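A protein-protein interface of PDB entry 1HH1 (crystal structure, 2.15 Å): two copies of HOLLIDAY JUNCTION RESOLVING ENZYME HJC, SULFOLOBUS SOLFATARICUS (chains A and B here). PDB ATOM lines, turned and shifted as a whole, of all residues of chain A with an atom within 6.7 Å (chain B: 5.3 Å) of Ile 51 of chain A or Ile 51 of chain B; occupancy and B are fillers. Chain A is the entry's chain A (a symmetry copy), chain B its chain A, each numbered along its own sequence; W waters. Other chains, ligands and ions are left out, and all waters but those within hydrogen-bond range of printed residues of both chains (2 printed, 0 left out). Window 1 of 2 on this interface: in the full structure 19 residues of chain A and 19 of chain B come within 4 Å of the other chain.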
ATOM      1  N   ILE A  44     -36.161  -2.458   5.933  1.00  0.00           N
ATOM      2  CA  ILE A  44     -34.880  -3.079   6.272  1.00  0.00           C
ATOM      3  C   ILE A  44     -35.174  -4.571   6.521  1.00  0.00           C
ATOM      4  O   ILE A  44     -35.988  -4.934   7.387  1.00  0.00           O
ATOM      5  CB  ILE A  44     -34.211  -2.416   7.482  1.00  0.00           C
ATOM      6  CG1 ILE A  44     -33.840  -0.983   7.100  1.00  0.00           C
ATOM      7  CG2 ILE A  44     -32.988  -3.188   7.973  1.00  0.00           C
ATOM      8  CD1 ILE A  44     -34.029   0.015   8.194  1.00  0.00           C
ATOM      9  N   ALA A  45     -34.551  -5.436   5.735  1.00  0.00           N
ATOM     10  CA  ALA A  45     -34.918  -6.863   5.828  1.00  0.00           C
ATOM     11  C   ALA A  45     -33.615  -7.651   6.014  1.00  0.00           C
ATOM     12  O   ALA A  45     -32.615  -7.461   5.329  1.00  0.00           O
ATOM     13  CB  ALA A  45     -35.709  -7.252   4.601  1.00  0.00           C
ATOM     14  N   LEU A  46     -33.640  -8.535   7.012  1.00  0.00           N
ATOM     15  CA  LEU A  46     -32.459  -9.283   7.387  1.00  0.00           C
ATOM     16  C   LEU A  46     -32.729 -10.777   7.367  1.00  0.00           C
ATOM     17  O   LEU A  46     -33.717 -11.211   7.940  1.00  0.00           O
ATOM     18  CB  LEU A  46     -32.062  -8.840   8.829  1.00  0.00           C
ATOM     19  CG  LEU A  46     -32.048  -7.343   9.160  1.00  0.00           C
ATOM     20  CD1 LEU A  46     -31.866  -7.099  10.675  1.00  0.00           C
ATOM     21  CD2 LEU A  46     -30.923  -6.569   8.457  1.00  0.00           C
ATOM     22  N   LYS A  47     -31.785 -11.565   6.863  1.00  0.00           N
ATOM     23  CA  LYS A  47     -31.945 -13.007   6.912  1.00  0.00           C
ATOM     24  C   LYS A  47     -30.585 -13.648   6.973  1.00  0.00           C
ATOM     25  O   LYS A  47     -29.733 -13.424   6.093  1.00  0.00           O
ATOM     26  CB  LYS A  47     -32.744 -13.537   5.710  1.00  0.00           C
ATOM     27  CG  LYS A  47     -32.998 -15.041   5.807  1.00  0.00           C
ATOM     28  CD  LYS A  47     -34.119 -15.485   4.839  1.00  0.00           C
ATOM     29  CE  LYS A  47     -34.280 -17.006   4.984  1.00  0.00           C
ATOM     30  NZ  LYS A  47     -35.333 -17.608   4.141  1.00  0.00           N
ATOM     31  N   ASN A  48     -30.387 -14.366   8.094  1.00  0.00           N
ATOM     32  CA  ASN A  48     -29.137 -15.080   8.272  1.00  0.00           C
ATOM     33  C   ASN A  48     -27.897 -14.308   7.866  1.00  0.00           C
ATOM     34  O   ASN A  48     -27.048 -14.841   7.140  1.00  0.00           O
ATOM     35  CB  ASN A  48     -29.193 -16.413   7.485  1.00  0.00           C
ATOM     36  CG  ASN A  48     -28.340 -17.517   8.104  1.00  0.00           C
ATOM     37  OD1 ASN A  48     -27.448 -17.289   8.910  1.00  0.00           O
ATOM     38  ND2 ASN A  48     -28.601 -18.773   7.741  1.00  0.00           N
ATOM     39  N   GLY A  49     -27.686 -13.136   8.462  1.00  0.00           N
ATOM     40  CA  GLY A  49     -26.483 -12.348   8.226  1.00  0.00           C
ATOM     41  C   GLY A  49     -26.556 -11.428   7.013  1.00  0.00           C
ATOM     42  O   GLY A  49     -25.628 -10.627   6.846  1.00  0.00           O
ATOM     43  N   VAL A  50     -27.559 -11.544   6.136  1.00  0.00           N
ATOM     44  CA  VAL A  50     -27.574 -10.702   4.924  1.00  0.00           C
ATOM     45  C   VAL A  50     -28.495  -9.520   5.102  1.00  0.00           C
ATOM     46  O   VAL A  50     -29.585  -9.720   5.644  1.00  0.00           O
ATOM     47  CB  VAL A  50     -28.012 -11.533   3.695  1.00  0.00           C
ATOM     48  CG1 VAL A  50     -28.037 -10.680   2.420  1.00  0.00           C
ATOM     49  CG2 VAL A  50     -27.017 -12.687   3.513  1.00  0.00           C
ATOM     50  N   ILE A  51     -28.068  -8.320   4.701  1.00  0.00           N
ATOM     51  CA  ILE A  51     -28.903  -7.138   4.860  1.00  0.00           C
ATOM     52  C   ILE A  51     -29.432  -6.622   3.504  1.00  0.00           C
ATOM     53  O   ILE A  51     -28.656  -6.403   2.578  1.00  0.00           O
ATOM     54  CB  ILE A  51     -28.065  -6.027   5.524  1.00  0.00           C
ATOM     55  CG1 ILE A  51     -27.540  -6.491   6.912  1.00  0.00           C
ATOM     56  CG2 ILE A  51     -28.851  -4.732   5.651  1.00  0.00           C
ATOM     57  CD1 ILE A  51     -26.239  -5.713   7.192  1.00  0.00           C
ATOM     58  N   ILE A  52     -30.747  -6.403   3.350  1.00  0.00           N
ATOM     59  CA  ILE A  52     -31.246  -5.800   2.121  1.00  0.00           C
ATOM     60  C   ILE A  52     -32.093  -4.620   2.591  1.00  0.00           C
ATOM     61  O   ILE A  52     -32.560  -4.622   3.728  1.00  0.00           O
ATOM     62  CB  ILE A  52     -31.963  -6.707   1.118  1.00  0.00           C
ATOM     63  CG1 ILE A  52     -33.175  -7.341   1.764  1.00  0.00           C
ATOM     64  CG2 ILE A  52     -30.997  -7.781   0.590  1.00  0.00           C
ATOM     65  CD1 ILE A  52     -34.069  -8.079   0.778  1.00  0.00           C
ATOM     66  N   LEU A  53     -32.066  -3.574   1.789  1.00  0.00           N
ATOM     67  CA  LEU A  53     -32.687  -2.300   2.070  1.00  0.00           C
ATOM     68  C   LEU A  53     -33.527  -1.969   0.828  1.00  0.00           C
ATOM     69  O   LEU A  53     -33.062  -2.042  -0.316  1.00  0.00           O
ATOM     70  CB  LEU A  53     -31.574  -1.242   2.246  1.00  0.00           C
ATOM     71  CG  LEU A  53     -30.489  -1.593   3.286  1.00  0.00           C
ATOM     72  CD1 LEU A  53     -29.259  -0.696   3.196  1.00  0.00           C
ATOM     73  CD2 LEU A  53     -31.111  -1.512   4.668  1.00  0.00           C
ATOM     74  N   PHE A  79     -26.892   5.243   4.167  1.00  0.00           N
ATOM     75  CA  PHE A  79     -27.326   4.197   5.115  1.00  0.00           C
ATOM     76  C   PHE A  79     -26.880   2.833   4.589  1.00  0.00           C
ATOM     77  O   PHE A  79     -26.305   1.974   5.280  1.00  0.00           O
ATOM     78  CB  PHE A  79     -28.834   4.290   5.339  1.00  0.00           C
ATOM     79  CG  PHE A  79     -29.390   3.404   6.400  1.00  0.00           C
ATOM     80  CD1 PHE A  79     -29.491   2.037   6.193  1.00  0.00           C
ATOM     81  CD2 PHE A  79     -29.800   3.915   7.607  1.00  0.00           C
ATOM     82  CE1 PHE A  79     -30.010   1.202   7.160  1.00  0.00           C
ATOM     83  CE2 PHE A  79     -30.319   3.095   8.606  1.00  0.00           C
ATOM     84  CZ  PHE A  79     -30.416   1.728   8.373  1.00  0.00           C
ATOM     85  N   SER A  83     -24.064   0.441   6.539  1.00  0.00           N
ATOM     86  CA  SER A  83     -24.568  -0.841   6.967  1.00  0.00           C
ATOM     87  C   SER A  83     -23.896  -2.003   6.238  1.00  0.00           C
ATOM     88  O   SER A  83     -23.922  -3.127   6.739  1.00  0.00           O
ATOM     89  CB  SER A  83     -26.088  -0.991   6.737  1.00  0.00           C
ATOM     90  OG  SER A  83     -26.459  -0.840   5.368  1.00  0.00           O
ATOM     91  N   GLY A  84     -23.445  -1.753   5.010  1.00  0.00           N
ATOM     92  CA  GLY A  84     -22.963  -2.805   4.132  1.00  0.00           C
ATOM     93  C   GLY A  84     -24.150  -3.578   3.517  1.00  0.00           C
ATOM     94  O   GLY A  84     -23.917  -4.630   2.933  1.00  0.00           O
ATOM     95  N   GLY A  85     -25.356  -3.057   3.548  1.00  0.00           N
ATOM     96  CA  GLY A  85     -26.565  -3.657   3.032  1.00  0.00           C
ATOM     97  C   GLY A  85     -26.755  -3.357   1.545  1.00  0.00           C
ATOM     98  O   GLY A  85     -26.168  -2.403   1.040  1.00  0.00           O
ATOM     99  N   SER A  86     -27.406  -4.259   0.830  1.00  0.00           N
ATOM    100  CA  SER A  86     -27.676  -4.066  -0.595  1.00  0.00           C
ATOM    101  C   SER A  86     -28.964  -3.259  -0.694  1.00  0.00           C
ATOM    102  O   SER A  86     -29.981  -3.646  -0.105  1.00  0.00           O
ATOM    103  CB  SER A  86     -27.804  -5.420  -1.317  1.00  0.00           C
ATOM    104  OG  SER A  86     -26.567  -6.112  -1.145  1.00  0.00           O
ATOM    105  N   LEU A  87     -28.936  -2.187  -1.444  1.00  0.00           N
ATOM    106  CA  LEU A  87     -30.067  -1.276  -1.592  1.00  0.00           C
ATOM    107  C   LEU A  87     -30.814  -1.453  -2.912  1.00  0.00           C
ATOM    108  O   LEU A  87     -30.246  -1.688  -3.975  1.00  0.00           O
ATOM    109  CB  LEU A  87     -29.540   0.166  -1.528  1.00  0.00           C
ATOM    110  CG  LEU A  87     -30.545   1.325  -1.674  1.00  0.00           C
ATOM    111  CD1 LEU A  87     -31.551   1.348  -0.551  1.00  0.00           C
ATOM    112  CD2 LEU A  87     -29.781   2.658  -1.707  1.00  0.00           C
ATOM    113  N   PHE A  88     -32.143  -1.392  -2.838  1.00  0.00           N
ATOM    114  CA  PHE A  88     -32.995  -1.611  -3.984  1.00  0.00           C
ATOM    115  C   PHE A  88     -34.141  -0.618  -3.964  1.00  0.00           C
ATOM    116  O   PHE A  88     -34.651  -0.241  -2.914  1.00  0.00           O
ATOM    117  CB  PHE A  88     -33.709  -3.002  -3.998  1.00  0.00           C
ATOM    118  CG  PHE A  88     -32.702  -4.114  -4.058  1.00  0.00           C
ATOM    119  CD1 PHE A  88     -32.106  -4.551  -2.875  1.00  0.00           C
ATOM    120  CD2 PHE A  88     -32.323  -4.688  -5.243  1.00  0.00           C
ATOM    121  CE1 PHE A  88     -31.151  -5.533  -2.897  1.00  0.00           C
ATOM    122  CE2 PHE A  88     -31.363  -5.674  -5.281  1.00  0.00           C
ATOM    123  CZ  PHE A  88     -30.766  -6.110  -4.102  1.00  0.00           C
ATOM    124  N   VAL A 131     -30.563 -12.991  -1.952  1.00  0.00           N
ATOM    125  CA  VAL A 131     -30.273 -13.126  -0.520  1.00  0.00           C
ATOM    126  C   VAL A 131     -29.881 -14.556  -0.178  1.00  0.00           C
ATOM    127  O   VAL A 131     -28.858 -14.833   0.461  1.00  0.00           O
ATOM    128  CB  VAL A 131     -31.471 -12.692   0.349  1.00  0.00           C
ATOM    129  CG1 VAL A 131     -31.183 -13.050   1.816  1.00  0.00           C
ATOM    130  CG2 VAL A 131     -31.758 -11.206   0.194  1.00  0.00           C
ATOM    131  N   LYS A 134     -26.342 -15.483  -1.244  1.00  0.00           N
ATOM    132  CA  LYS A 134     -25.269 -14.918  -0.396  1.00  0.00           C
ATOM    133  C   LYS A 134     -25.189 -15.738   0.896  1.00  0.00           C
ATOM    134  O   LYS A 134     -24.102 -15.991   1.399  1.00  0.00           O
ATOM    135  CB  LYS A 134     -25.527 -13.448  -0.045  1.00  0.00           C
ATOM    136  CG  LYS A 134     -25.471 -12.528  -1.253  1.00  0.00           C
ATOM    137  CD  LYS A 134     -26.014 -11.134  -1.023  1.00  0.00           C
ATOM    138  CE  LYS A 134     -25.447 -10.161  -2.059  1.00  0.00           C
ATOM    139  NZ  LYS A 134     -25.968  -8.784  -1.830  1.00  0.00           N
ATOM    140  N   ILE B  44     -31.679  -1.543  16.221  1.00  0.00           N
ATOM    141  CA  ILE B  44     -31.067  -2.379  15.187  1.00  0.00           C
ATOM    142  C   ILE B  44     -29.890  -1.567  14.614  1.00  0.00           C
ATOM    143  O   ILE B  44     -30.063  -0.444  14.111  1.00  0.00           O
ATOM    144  CB  ILE B  44     -32.067  -2.787  14.099  1.00  0.00           C
ATOM    145  CG1 ILE B  44     -33.123  -3.693  14.733  1.00  0.00           C
ATOM    146  CG2 ILE B  44     -31.394  -3.474  12.912  1.00  0.00           C
ATOM    147  CD1 ILE B  44     -34.507  -3.480  14.217  1.00  0.00           C
ATOM    148  N   ALA B  45     -28.686  -2.107  14.730  1.00  0.00           N
ATOM    149  CA  ALA B  45     -27.511  -1.302  14.340  1.00  0.00           C
ATOM    150  C   ALA B  45     -26.682  -2.155  13.371  1.00  0.00           C
ATOM    151  O   ALA B  45     -26.403  -3.330  13.586  1.00  0.00           O
ATOM    152  CB  ALA B  45     -26.769  -0.876  15.585  1.00  0.00           C
ATOM    153  N   LEU B  46     -26.323  -1.528  12.250  1.00  0.00           N
ATOM    154  CA  LEU B  46     -25.630  -2.222  11.187  1.00  0.00           C
ATOM    155  C   LEU B  46     -24.333  -1.520  10.830  1.00  0.00           C
ATOM    156  O   LEU B  46     -24.346  -0.315  10.624  1.00  0.00           O
ATOM    157  CB  LEU B  46     -26.575  -2.244   9.946  1.00  0.00           C
ATOM    158  CG  LEU B  46     -28.047  -2.618  10.150  1.00  0.00           C
ATOM    159  CD1 LEU B  46     -28.880  -2.361   8.875  1.00  0.00           C
ATOM    160  CD2 LEU B  46     -28.261  -4.094  10.519  1.00  0.00           C
ATOM    161  N   GLY B  49     -21.899  -4.915   6.990  1.00  0.00           N
ATOM    162  CA  GLY B  49     -22.311  -6.311   6.935  1.00  0.00           C
ATOM    163  C   GLY B  49     -22.627  -6.933   8.290  1.00  0.00           C
ATOM    164  O   GLY B  49     -23.123  -8.066   8.299  1.00  0.00           O
ATOM    165  N   VAL B  50     -22.309  -6.289   9.420  1.00  0.00           N
ATOM    166  CA  VAL B  50     -22.546  -6.937  10.723  1.00  0.00           C
ATOM    167  C   VAL B  50     -23.820  -6.429  11.352  1.00  0.00           C
ATOM    168  O   VAL B  50     -24.045  -5.217  11.293  1.00  0.00           O
ATOM    169  CB  VAL B  50     -21.352  -6.688  11.676  1.00  0.00           C
ATOM    170  CG1 VAL B  50     -21.574  -7.350  13.041  1.00  0.00           C
ATOM    171  CG2 VAL B  50     -20.090  -7.272  11.028  1.00  0.00           C
ATOM    172  N   ILE B  51     -24.652  -7.318  11.902  1.00  0.00           N
ATOM    173  CA  ILE B  51     -25.905  -6.893  12.510  1.00  0.00           C
ATOM    174  C   ILE B  51     -25.872  -7.027  14.048  1.00  0.00           C
ATOM    175  O   ILE B  51     -25.551  -8.091  14.570  1.00  0.00           O
ATOM    176  CB  ILE B  51     -27.046  -7.771  11.956  1.00  0.00           C
ATOM    177  CG1 ILE B  51     -27.139  -7.639  10.410  1.00  0.00           C
ATOM    178  CG2 ILE B  51     -28.377  -7.436  12.607  1.00  0.00           C
ATOM    179  CD1 ILE B  51     -27.746  -8.952   9.875  1.00  0.00           C
ATOM    180  N   ILE B  52     -26.210  -5.974  14.808  1.00  0.00           N
ATOM    181  CA  ILE B  52     -26.303  -6.122  16.255  1.00  0.00           C
ATOM    182  C   ILE B  52     -27.688  -5.583  16.604  1.00  0.00           C
ATOM    183  O   ILE B  52     -28.244  -4.794  15.844  1.00  0.00           O
ATOM    184  CB  ILE B  52     -25.182  -5.526  17.110  1.00  0.00           C
ATOM    185  CG1 ILE B  52     -25.083  -4.035  16.872  1.00  0.00           C
ATOM    186  CG2 ILE B  52     -23.847  -6.222  16.792  1.00  0.00           C
ATOM    187  CD1 ILE B  52     -24.147  -3.329  17.842  1.00  0.00           C
ATOM    188  N   LEU B  53     -28.275  -6.198  17.612  1.00  0.00           N
ATOM    189  CA  LEU B  53     -29.628  -5.953  18.056  1.00  0.00           C
ATOM    190  C   LEU B  53     -29.528  -5.715  19.570  1.00  0.00           C
ATOM    191  O   LEU B  53     -28.903  -6.480  20.313  1.00  0.00           O
ATOM    192  CB  LEU B  53     -30.470  -7.220  17.781  1.00  0.00           C
ATOM    193  CG  LEU B  53     -30.429  -7.736  16.327  1.00  0.00           C
ATOM    194  CD1 LEU B  53     -30.995  -9.143  16.174  1.00  0.00           C
ATOM    195  CD2 LEU B  53     -31.186  -6.755  15.452  1.00  0.00           C
ATOM    196  N   SER B  83     -32.610 -13.036  11.515  1.00  0.00           N
ATOM    197  CA  SER B  83     -31.728 -12.044  10.949  1.00  0.00           C
ATOM    198  C   SER B  83     -30.277 -12.517  10.897  1.00  0.00           C
ATOM    199  O   SER B  83     -29.492 -11.977  10.119  1.00  0.00           O
ATOM    200  CB  SER B  83     -31.737 -10.718  11.739  1.00  0.00           C
ATOM    201  OG  SER B  83     -31.349 -10.883  13.102  1.00  0.00           O
ATOM    202  N   GLY B  84     -29.906 -13.399  11.824  1.00  0.00           N
ATOM    203  CA  GLY B  84     -28.519 -13.786  12.016  1.00  0.00           C
ATOM    204  C   GLY B  84     -27.756 -12.686  12.787  1.00  0.00           C
ATOM    205  O   GLY B  84     -26.534 -12.754  12.837  1.00  0.00           O
ATOM    206  N   GLY B  85     -28.424 -11.765  13.444  1.00  0.00           N
ATOM    207  CA  GLY B  85     -27.861 -10.668  14.197  1.00  0.00           C
ATOM    208  C   GLY B  85     -27.526 -11.079  15.631  1.00  0.00           C
ATOM    209  O   GLY B  85     -28.068 -12.068  16.119  1.00  0.00           O
ATOM    210  N   SER B  86     -26.522 -10.450  16.216  1.00  0.00           N
ATOM    211  CA  SER B  86     -26.129 -10.736  17.596  1.00  0.00           C
ATOM    212  C   SER B  86     -27.010  -9.875  18.492  1.00  0.00           C
ATOM    213  O   SER B  86     -27.077  -8.654  18.300  1.00  0.00           O
ATOM    214  CB  SER B  86     -24.636 -10.433  17.817  1.00  0.00           C
ATOM    215  OG  SER B  86     -23.897 -11.263  16.919  1.00  0.00           O
HETATM  216  O   HOH W   1     -23.793 -10.603   8.964  1.00  0.00           O
HETATM  217  O   HOH W   2     -23.755  -9.016   5.739  1.00  0.00           O
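The backbone NH of Gly 49 of chain B is in hydrogen-bond range of the backbone carbonyl oxygen of Ser 83 of chain A, 2.7 Å away. N of Asn 48 of chain A lies within hydrogen-bond range of O of Ser 83 of chain B (3.3 Å). O of Ser 83 of chain B is in hydrogen-bond range of N of Gly 49 of chain A (2.7 Å).
The backbone NH (N) of Ser 86 of chain B sits at hydrogen-bond distance from the backbone carbonyl oxygen (O) of Ile 51 of chain B, at 3.0 Å. OG of Ser 83 of chain B is in hydrogen-bond range of N of Gly 85 of chain B (3.1 Å). The backbone NH of Ser 86 of chain A sits at hydrogen-bond distance from the backbone carbonyl oxygen of Ile 51 of chain A (3.0 Å). The backbone carbonyl oxygen of Phe 79 of chain A sits at hydrogen-bond distance from the side-chain hydroxyl of Ser 83 of chain A, 2.8 Å away. The backbone NH of Gly 85 of chain A lies within hydrogen-bond range of the side-chain hydroxyl of Ser 83 of chain A (3.1 Å).
Among the printed residues, pairs that only touch across the chains: Leu 46 of chain A with Ser 83 of chain B, Lys 47 of chain A with Ser 83 of chain B, Asn 48 of chain A with Gly 84 of chain B, Gly 49 of chain A with Gly 49 of chain B, Gly 49 of chain A with Ile 51 of chain B, Gly 49 of chain A with Gly 84 of chain B, Ile 51 of chain A with Gly 49 of chain B, Ile 51 of chain A with Ile 51 of chain B, Ser 83 of chain A with Leu 46 of chain B and Gly 84 of chain A with Gly 49 of chain B.
Printed residues of chain A within 4 Å of Ile 51 of chain B: Gly 49 (3.97 Å) and Ile 51 (3.7 Å). Of the printed residues of chain B, Leu 46 of chain A touches Ser 83 (3.5 Å). Of the printed residues of chain B, Ser 83 of chain A touches Leu 46 (3.5 Å) and Gly 49 (2.7 Å). Leu 87 of chain A touches none of the printed residues of chain B. Ser 86 of chain B touches none of the printed residues of chain A. The nearest printed residue of chain A that does not touch Ile 51 of chain B is Leu 46 of chain A (4.002 Å). The nearest printed residue of chain B that does not touch Lys 47 of chain A is Gly 84 of chain B (4.9 Å).
Hydrophobic or aromatic side chains of chain A that line the printed part of chain B: Leu 46 and Ile 51. Of the 12 printed residues of chain B, 5 touch a printed residue of chain A. Printed residues of chain B that touch a printed residue of chain A: Leu 46, Gly 49, Ile 51, Ser 83 and Gly 84. Along chain B the printed residues that touch a printed residue of chain A span positions 46 to 84. Among the printed residues, 13 pairs touch across the chains. Among the printed residues, no Asp or Glu carboxylate lies within 4 Å of a Lys or Arg side-chain nitrogen of the other chain.
Leu 46 of chain A touches Ser 83 of chain B, and with the chains exchanged Ser 83 of chain A touches Leu 46 of chain B. Gly 49 of chain A touches Ile 51 of chain B, and with the chains exchanged Ile 51 of chain A touches Gly 49 of chain B. Gly 49 of chain A touches Ser 83 of chain B, and with the chains exchanged Ser 83 of chain A touches Gly 49 of chain B. Ile 51 of chain A touches its own counterpart, Ile 51 of chain B. Positions printed for both chains: 44, 45, 46, 49, 50, 51, 52, 53, 83, 84, 85 and 86.
Water W1 lies within hydrogen-bond range of O of Gly 49 of chain B (2.7 Å) and O of Gly 49 of chain A (2.8 Å). Water W2 lies within hydrogen-bond range of the backbone carbonyl oxygen of Gly 49 of chain A and the backbone carbonyl oxygen of Gly 49 of chain B.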
